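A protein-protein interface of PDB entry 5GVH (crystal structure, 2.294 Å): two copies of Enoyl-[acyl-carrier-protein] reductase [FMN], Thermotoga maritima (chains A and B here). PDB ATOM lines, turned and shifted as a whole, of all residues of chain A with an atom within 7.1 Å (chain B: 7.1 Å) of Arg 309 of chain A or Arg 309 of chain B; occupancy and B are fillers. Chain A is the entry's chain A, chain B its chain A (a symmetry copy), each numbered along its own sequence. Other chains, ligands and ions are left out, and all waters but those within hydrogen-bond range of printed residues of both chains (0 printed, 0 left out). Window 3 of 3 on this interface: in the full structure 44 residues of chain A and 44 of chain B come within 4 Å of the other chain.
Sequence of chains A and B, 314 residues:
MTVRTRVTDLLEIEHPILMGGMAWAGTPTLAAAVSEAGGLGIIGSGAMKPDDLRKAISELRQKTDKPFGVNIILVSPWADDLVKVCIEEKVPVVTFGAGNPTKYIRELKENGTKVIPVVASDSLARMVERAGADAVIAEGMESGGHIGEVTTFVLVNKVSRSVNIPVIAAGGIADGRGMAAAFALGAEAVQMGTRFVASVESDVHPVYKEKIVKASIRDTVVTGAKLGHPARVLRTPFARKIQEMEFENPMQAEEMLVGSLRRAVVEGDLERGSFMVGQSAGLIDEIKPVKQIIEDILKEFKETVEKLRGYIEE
The guanidinium group of Arg 309 of chain B sits close to the guanidinium group of Arg 309 of chain A, at 2.8 Å.
Leu 308 of chain B touches Val 305 of chain A (O to CG1, 3.6 Å). Val 305 of chain A touches Arg 309 of chain B. O of Leu 308 of chain A touches CG1 of Val 305 of chain B (3.6 Å). Leu 308 of chain A touches Leu 308 of chain B. Arg 309 of chain A touches Val 305 of chain B (N to CG1, 3.9 Å).
Arg 309 of chain A touches two residues of chain B. Arg 309 of chain B touches just these residues of chain A: Val 305 and Arg 309. Printed residues of chain A within 4 Å of Leu 308 of chain B: Val 305 (3.6 Å) and Leu 308 (3.7 Å). Printed residues of chain B within 4 Å of Val 305 of chain A: Leu 308 (3.6 Å) and Arg 309 (3.9 Å). Of the printed residues of chain A, Val 305 of chain B touches Leu 308 and Arg 309. Of the printed residues of chain B, Leu 308 of chain A touches Val 305 (3.6 Å) and Leu 308 (3.7 Å). Glu 303 of chain A touches none of the printed residues of chain B. Tyr 311 of chain A touches none of the printed residues of chain B. The nearest printed residue of chain A that does not touch Val 305 of chain B is Ile 312 of chain A (4.4 Å).
Printed residues of chain A that touch a printed residue of chain B: Val 305, Leu 308 and Arg 309. Hydrophobic or aromatic side chains of chain A within 4 Å of the printed part of chain B: Val 305 and Leu 308. Printed residues of chain B that touch a printed residue of chain A: Val 305, Leu 308 and Arg 309. Hydrophobic or aromatic side chains of chain B that line the printed part of chain A: Val 305 and Leu 308.
Val 305 of chain A touches Leu 308 of chain B, and with the chains exchanged Leu 308 of chain A touches Val 305 of chain B. Val 305 of chain A touches Arg 309 of chain B, and with the chains exchanged Arg 309 of chain A touches Val 305 of chain B. Leu 308 of chain A touches its own counterpart, Leu 308 of chain B. Arg 309 of chain A touches its own counterpart, Arg 309 of chain B. 10 positions are printed for both chains. Of the 6 pairs that touch across the chains among the printed residues, 6 have their exchanged pair printed and touching as well.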
ATOM      1  N   GLU A 303      34.557   7.762  -9.952  1.00  0.00           N
ATOM      2  CA  GLU A 303      33.831   6.508  -9.774  1.00  0.00           C
ATOM      3  C   GLU A 303      32.878   6.574  -8.587  1.00  0.00           C
ATOM      4  O   GLU A 303      31.807   5.955  -8.620  1.00  0.00           O
ATOM      5  CB  GLU A 303      34.806   5.342  -9.599  1.00  0.00           C
ATOM      6  CG  GLU A 303      36.066   5.434 -10.436  1.00  0.00           C
ATOM      7  CD  GLU A 303      37.072   4.341 -10.105  1.00  0.00           C
ATOM      8  OE1 GLU A 303      37.180   3.372 -10.890  1.00  0.00           O
ATOM      9  OE2 GLU A 303      37.749   4.445  -9.055  1.00  0.00           O
ATOM     10  N   THR A 304      33.241   7.318  -7.536  1.00  0.00           N
ATOM     11  CA  THR A 304      32.337   7.467  -6.401  1.00  0.00           C
ATOM     12  C   THR A 304      31.090   8.253  -6.794  1.00  0.00           C
ATOM     13  O   THR A 304      29.980   7.931  -6.349  1.00  0.00           O
ATOM     14  CB  THR A 304      33.057   8.135  -5.225  1.00  0.00           C
ATOM     15  OG1 THR A 304      34.232   7.384  -4.885  1.00  0.00           O
ATOM     16  CG2 THR A 304      32.140   8.205  -3.997  1.00  0.00           C
ATOM     17  N   VAL A 305      31.244   9.275  -7.644  1.00  0.00           N
ATOM     18  CA  VAL A 305      30.074  10.042  -8.071  1.00  0.00           C
ATOM     19  C   VAL A 305      29.134   9.168  -8.904  1.00  0.00           C
ATOM     20  O   VAL A 305      27.909   9.250  -8.760  1.00  0.00           O
ATOM     21  CB  VAL A 305      30.512  11.317  -8.822  1.00  0.00           C
ATOM     22  CG1 VAL A 305      29.312  12.128  -9.278  1.00  0.00           C
ATOM     23  CG2 VAL A 305      31.385  12.179  -7.925  1.00  0.00           C
ATOM     24  N   GLU A 306      29.685   8.302  -9.768  1.00  0.00           N
ATOM     25  CA  GLU A 306      28.842   7.399 -10.557  1.00  0.00           C
ATOM     26  C   GLU A 306      28.088   6.422  -9.665  1.00  0.00           C
ATOM     27  O   GLU A 306      26.930   6.092  -9.944  1.00  0.00           O
ATOM     28  CB  GLU A 306      29.679   6.629 -11.585  1.00  0.00           C
ATOM     29  CG  GLU A 306      30.819   7.426 -12.179  1.00  0.00           C
ATOM     30  CD  GLU A 306      31.528   6.714 -13.321  1.00  0.00           C
ATOM     31  OE1 GLU A 306      32.236   5.716 -13.061  1.00  0.00           O
ATOM     32  OE2 GLU A 306      31.394   7.174 -14.476  1.00  0.00           O
ATOM     33  N   LYS A 307      28.730   5.936  -8.597  1.00  0.00           N
ATOM     34  CA  LYS A 307      28.029   5.074  -7.649  1.00  0.00           C
ATOM     35  C   LYS A 307      26.902   5.836  -6.963  1.00  0.00           C
ATOM     36  O   LYS A 307      25.762   5.364  -6.915  1.00  0.00           O
ATOM     37  CB  LYS A 307      29.014   4.494  -6.631  1.00  0.00           C
ATOM     38  CG  LYS A 307      28.381   3.782  -5.428  1.00  0.00           C
ATOM     39  CD  LYS A 307      27.245   2.825  -5.809  1.00  0.00           C
ATOM     40  CE  LYS A 307      27.728   1.602  -6.584  1.00  0.00           C
ATOM     41  NZ  LYS A 307      27.868   0.399  -5.709  1.00  0.00           N
ATOM     42  N   LEU A 308      27.197   7.030  -6.441  1.00  0.00           N
ATOM     43  CA  LEU A 308      26.138   7.854  -5.863  1.00  0.00           C
ATOM     44  C   LEU A 308      25.010   8.074  -6.859  1.00  0.00           C
ATOM     45  O   LEU A 308      23.837   8.108  -6.478  1.00  0.00           O
ATOM     46  CB  LEU A 308      26.705   9.196  -5.394  1.00  0.00           C
ATOM     47  CG  LEU A 308      27.788   9.092  -4.317  1.00  0.00           C
ATOM     48  CD1 LEU A 308      28.194  10.456  -3.755  1.00  0.00           C
ATOM     49  CD2 LEU A 308      27.322   8.165  -3.210  1.00  0.00           C
ATOM     50  N   ARG A 309      25.346   8.203  -8.139  1.00  0.00           N
ATOM     51  CA  ARG A 309      24.321   8.330  -9.164  1.00  0.00           C
ATOM     52  C   ARG A 309      23.462   7.078  -9.266  1.00  0.00           C
ATOM     53  O   ARG A 309      22.250   7.173  -9.504  1.00  0.00           O
ATOM     54  CB  ARG A 309      24.971   8.626 -10.504  1.00  0.00           C
ATOM     55  CG  ARG A 309      24.001   8.557 -11.653  1.00  0.00           C
ATOM     56  CD  ARG A 309      24.691   7.882 -12.807  1.00  0.00           C
ATOM     57  NE  ARG A 309      25.838   8.681 -13.218  1.00  0.00           N
ATOM     58  CZ  ARG A 309      25.780   9.731 -14.031  1.00  0.00           C
ATOM     59  NH1 ARG A 309      24.636  10.108 -14.581  1.00  0.00           N
ATOM     60  NH2 ARG A 309      26.884  10.398 -14.312  1.00  0.00           N
ATOM     61  N   GLY A 310      24.071   5.899  -9.101  1.00  0.00           N
ATOM     62  CA  GLY A 310      23.345   4.642  -9.189  1.00  0.00           C
ATOM     63  C   GLY A 310      22.122   4.555  -8.292  1.00  0.00           C
ATOM     64  O   GLY A 310      21.225   3.749  -8.563  1.00  0.00           O
ATOM     65  N   TYR A 311      22.057   5.377  -7.243  1.00  0.00           N
ATOM     66  CA  TYR A 311      20.921   5.404  -6.330  1.00  0.00           C
ATOM     67  C   TYR A 311      19.781   6.294  -6.821  1.00  0.00           C
ATOM     68  O   TYR A 311      18.862   6.586  -6.048  1.00  0.00           O
ATOM     69  CB  TYR A 311      21.374   5.854  -4.934  1.00  0.00           C
ATOM     70  CG  TYR A 311      22.327   4.885  -4.254  1.00  0.00           C
ATOM     71  CD1 TYR A 311      23.655   5.231  -4.014  1.00  0.00           C
ATOM     72  CD2 TYR A 311      21.897   3.620  -3.852  1.00  0.00           C
ATOM     73  CE1 TYR A 311      24.526   4.347  -3.394  1.00  0.00           C
ATOM     74  CE2 TYR A 311      22.763   2.728  -3.233  1.00  0.00           C
ATOM     75  CZ  TYR A 311      24.071   3.096  -3.008  1.00  0.00           C
ATOM     76  OH  TYR A 311      24.921   2.202  -2.397  1.00  0.00           O
ATOM     77  N   ILE A 312      19.821   6.744  -8.073  1.00  0.00           N
ATOM     78  CA  ILE A 312      18.681   7.451  -8.653  1.00  0.00           C
ATOM     79  C   ILE A 312      18.371   6.939 -10.063  1.00  0.00           C
ATOM     80  O   ILE A 312      19.200   7.026 -10.972  1.00  0.00           O
ATOM     81  CB  ILE A 312      18.909   8.962  -8.670  1.00  0.00           C
ATOM     82  CG1 ILE A 312      19.054   9.491  -7.243  1.00  0.00           C
ATOM     83  CG2 ILE A 312      17.743   9.648  -9.353  1.00  0.00           C
ATOM     84  CD1 ILE A 312      19.472  10.937  -7.173  1.00  0.00           C
ATOM     85  N   GLU B 303      19.449  16.201  -4.426  1.00  0.00           N
ATOM     86  CA  GLU B 303      20.008  17.418  -5.005  1.00  0.00           C
ATOM     87  C   GLU B 303      21.522  17.474  -4.843  1.00  0.00           C
ATOM     88  O   GLU B 303      22.216  18.012  -5.715  1.00  0.00           O
ATOM     89  CB  GLU B 303      19.368  18.658  -4.374  1.00  0.00           C
ATOM     90  CG  GLU B 303      17.893  18.519  -4.054  1.00  0.00           C
ATOM     91  CD  GLU B 303      17.346  19.711  -3.281  1.00  0.00           C
ATOM     92  OE1 GLU B 303      16.655  20.555  -3.897  1.00  0.00           O
ATOM     93  OE2 GLU B 303      17.614  19.811  -2.060  1.00  0.00           O
ATOM     94  N   THR B 304      22.053  16.923  -3.746  1.00  0.00           N
ATOM     95  CA  THR B 304      23.501  16.892  -3.573  1.00  0.00           C
ATOM     96  C   THR B 304      24.155  15.977  -4.604  1.00  0.00           C
ATOM     97  O   THR B 304      25.233  16.293  -5.127  1.00  0.00           O
ATOM     98  CB  THR B 304      23.862  16.458  -2.149  1.00  0.00           C
ATOM     99  OG1 THR B 304      23.224  17.325  -1.199  1.00  0.00           O
ATOM    100  CG2 THR B 304      25.380  16.518  -1.932  1.00  0.00           C
ATOM    101  N   VAL B 305      23.513  14.850  -4.929  1.00  0.00           N
ATOM    102  CA  VAL B 305      24.088  13.954  -5.932  1.00  0.00           C
ATOM    103  C   VAL B 305      24.110  14.630  -7.305  1.00  0.00           C
ATOM    104  O   VAL B 305      25.082  14.493  -8.056  1.00  0.00           O
ATOM    105  CB  VAL B 305      23.329  12.610  -5.951  1.00  0.00           C
ATOM    106  CG1 VAL B 305      23.909  11.665  -6.988  1.00  0.00           C
ATOM    107  CG2 VAL B 305      23.399  11.952  -4.583  1.00  0.00           C
ATOM    108  N   GLU B 306      23.056  15.387  -7.648  1.00  0.00           N
ATOM    109  CA  GLU B 306      23.040  16.104  -8.926  1.00  0.00           C
ATOM    110  C   GLU B 306      24.140  17.156  -8.988  1.00  0.00           C
ATOM    111  O   GLU B 306      24.741  17.366 -10.047  1.00  0.00           O
ATOM    112  CB  GLU B 306      21.675  16.760  -9.166  1.00  0.00           C
ATOM    113  CG  GLU B 306      20.501  15.957  -8.654  1.00  0.00           C
ATOM    114  CD  GLU B 306      19.151  16.530  -9.055  1.00  0.00           C
ATOM    115  OE1 GLU B 306      18.770  17.599  -8.527  1.00  0.00           O
ATOM    116  OE2 GLU B 306      18.461  15.892  -9.880  1.00  0.00           O
ATOM    117  N   LYS B 307      24.407  17.839  -7.869  1.00  0.00           N
ATOM    118  CA  LYS B 307      25.516  18.789  -7.837  1.00  0.00           C
ATOM    119  C   LYS B 307      26.844  18.071  -8.039  1.00  0.00           C
ATOM    120  O   LYS B 307      27.654  18.471  -8.880  1.00  0.00           O
ATOM    121  CB  LYS B 307      25.500  19.579  -6.525  1.00  0.00           C
ATOM    122  CG  LYS B 307      26.749  20.424  -6.246  1.00  0.00           C
ATOM    123  CD  LYS B 307      27.224  21.238  -7.456  1.00  0.00           C
ATOM    124  CE  LYS B 307      26.259  22.356  -7.839  1.00  0.00           C
ATOM    125  NZ  LYS B 307      26.700  23.685  -7.317  1.00  0.00           N
ATOM    126  N   LEU B 308      27.079  16.991  -7.288  1.00  0.00           N
ATOM    127  CA  LEU B 308      28.287  16.199  -7.507  1.00  0.00           C
ATOM    128  C   LEU B 308      28.397  15.759  -8.958  1.00  0.00           C
ATOM    129  O   LEU B 308      29.496  15.709  -9.516  1.00  0.00           O
ATOM    130  CB  LEU B 308      28.302  14.983  -6.579  1.00  0.00           C
ATOM    131  CG  LEU B 308      28.288  15.319  -5.085  1.00  0.00           C
ATOM    132  CD1 LEU B 308      28.483  14.084  -4.202  1.00  0.00           C
ATOM    133  CD2 LEU B 308      29.338  16.372  -4.787  1.00  0.00           C
ATOM    134  N   ARG B 309      27.266  15.459  -9.590  1.00  0.00           N
ATOM    135  CA  ARG B 309      27.277  15.112 -11.004  1.00  0.00           C
ATOM    136  C   ARG B 309      27.733  16.277 -11.870  1.00  0.00           C
ATOM    137  O   ARG B 309      28.428  16.070 -12.874  1.00  0.00           O
ATOM    138  CB  ARG B 309      25.891  14.657 -11.430  1.00  0.00           C
ATOM    139  CG  ARG B 309      25.764  14.489 -12.920  1.00  0.00           C
ATOM    140  CD  ARG B 309      24.421  15.023 -13.336  1.00  0.00           C
ATOM    141  NE  ARG B 309      23.371  14.245 -12.692  1.00  0.00           N
ATOM    142  CZ  ARG B 309      22.905  13.082 -13.137  1.00  0.00           C
ATOM    143  NH1 ARG B 309      23.351  12.553 -14.266  1.00  0.00           N
ATOM    144  NH2 ARG B 309      21.969  12.451 -12.453  1.00  0.00           N
ATOM    145  N   GLY B 310      27.343  17.504 -11.506  1.00  0.00           N
ATOM    146  CA  GLY B 310      27.715  18.684 -12.270  1.00  0.00           C
ATOM    147  C   GLY B 310      29.206  18.829 -12.523  1.00  0.00           C
ATOM    148  O   GLY B 310      29.598  19.526 -13.465  1.00  0.00           O
ATOM    149  N   TYR B 311      30.043  18.174 -11.716  1.00  0.00           N
ATOM    150  CA  TYR B 311      31.491  18.214 -11.879  1.00  0.00           C
ATOM    151  C   TYR B 311      32.008  17.189 -12.887  1.00  0.00           C
ATOM    152  O   TYR B 311      33.220  16.961 -12.954  1.00  0.00           O
ATOM    153  CB  TYR B 311      32.183  18.011 -10.524  1.00  0.00           C
ATOM    154  CG  TYR B 311      31.927  19.131  -9.528  1.00  0.00           C
ATOM    155  CD1 TYR B 311      31.178  18.911  -8.374  1.00  0.00           C
ATOM    156  CD2 TYR B 311      32.434  20.413  -9.746  1.00  0.00           C
ATOM    157  CE1 TYR B 311      30.944  19.932  -7.465  1.00  0.00           C
ATOM    158  CE2 TYR B 311      32.201  21.442  -8.842  1.00  0.00           C
ATOM    159  CZ  TYR B 311      31.458  21.197  -7.708  1.00  0.00           C
ATOM    160  OH  TYR B 311      31.230  22.225  -6.822  1.00  0.00           O
ATOM    161  N   ILE B 312      31.126  16.558 -13.658  1.00  0.00           N
ATOM    162  CA  ILE B 312      31.568  15.700 -14.755  1.00  0.00           C
ATOM    163  C   ILE B 312      30.762  15.970 -16.030  1.00  0.00           C
ATOM    164  O   ILE B 312      29.541  15.799 -16.063  1.00  0.00           O
ATOM    165  CB  ILE B 312      31.490  14.221 -14.377  1.00  0.00           C
ATOM    166  CG1 ILE B 312      32.427  13.926 -13.205  1.00  0.00           C
ATOM    167  CG2 ILE B 312      31.877  13.367 -15.566  1.00  0.00           C
ATOM    168  CD1 ILE B 312      32.272  12.536 -12.641  1.00  0.00           C
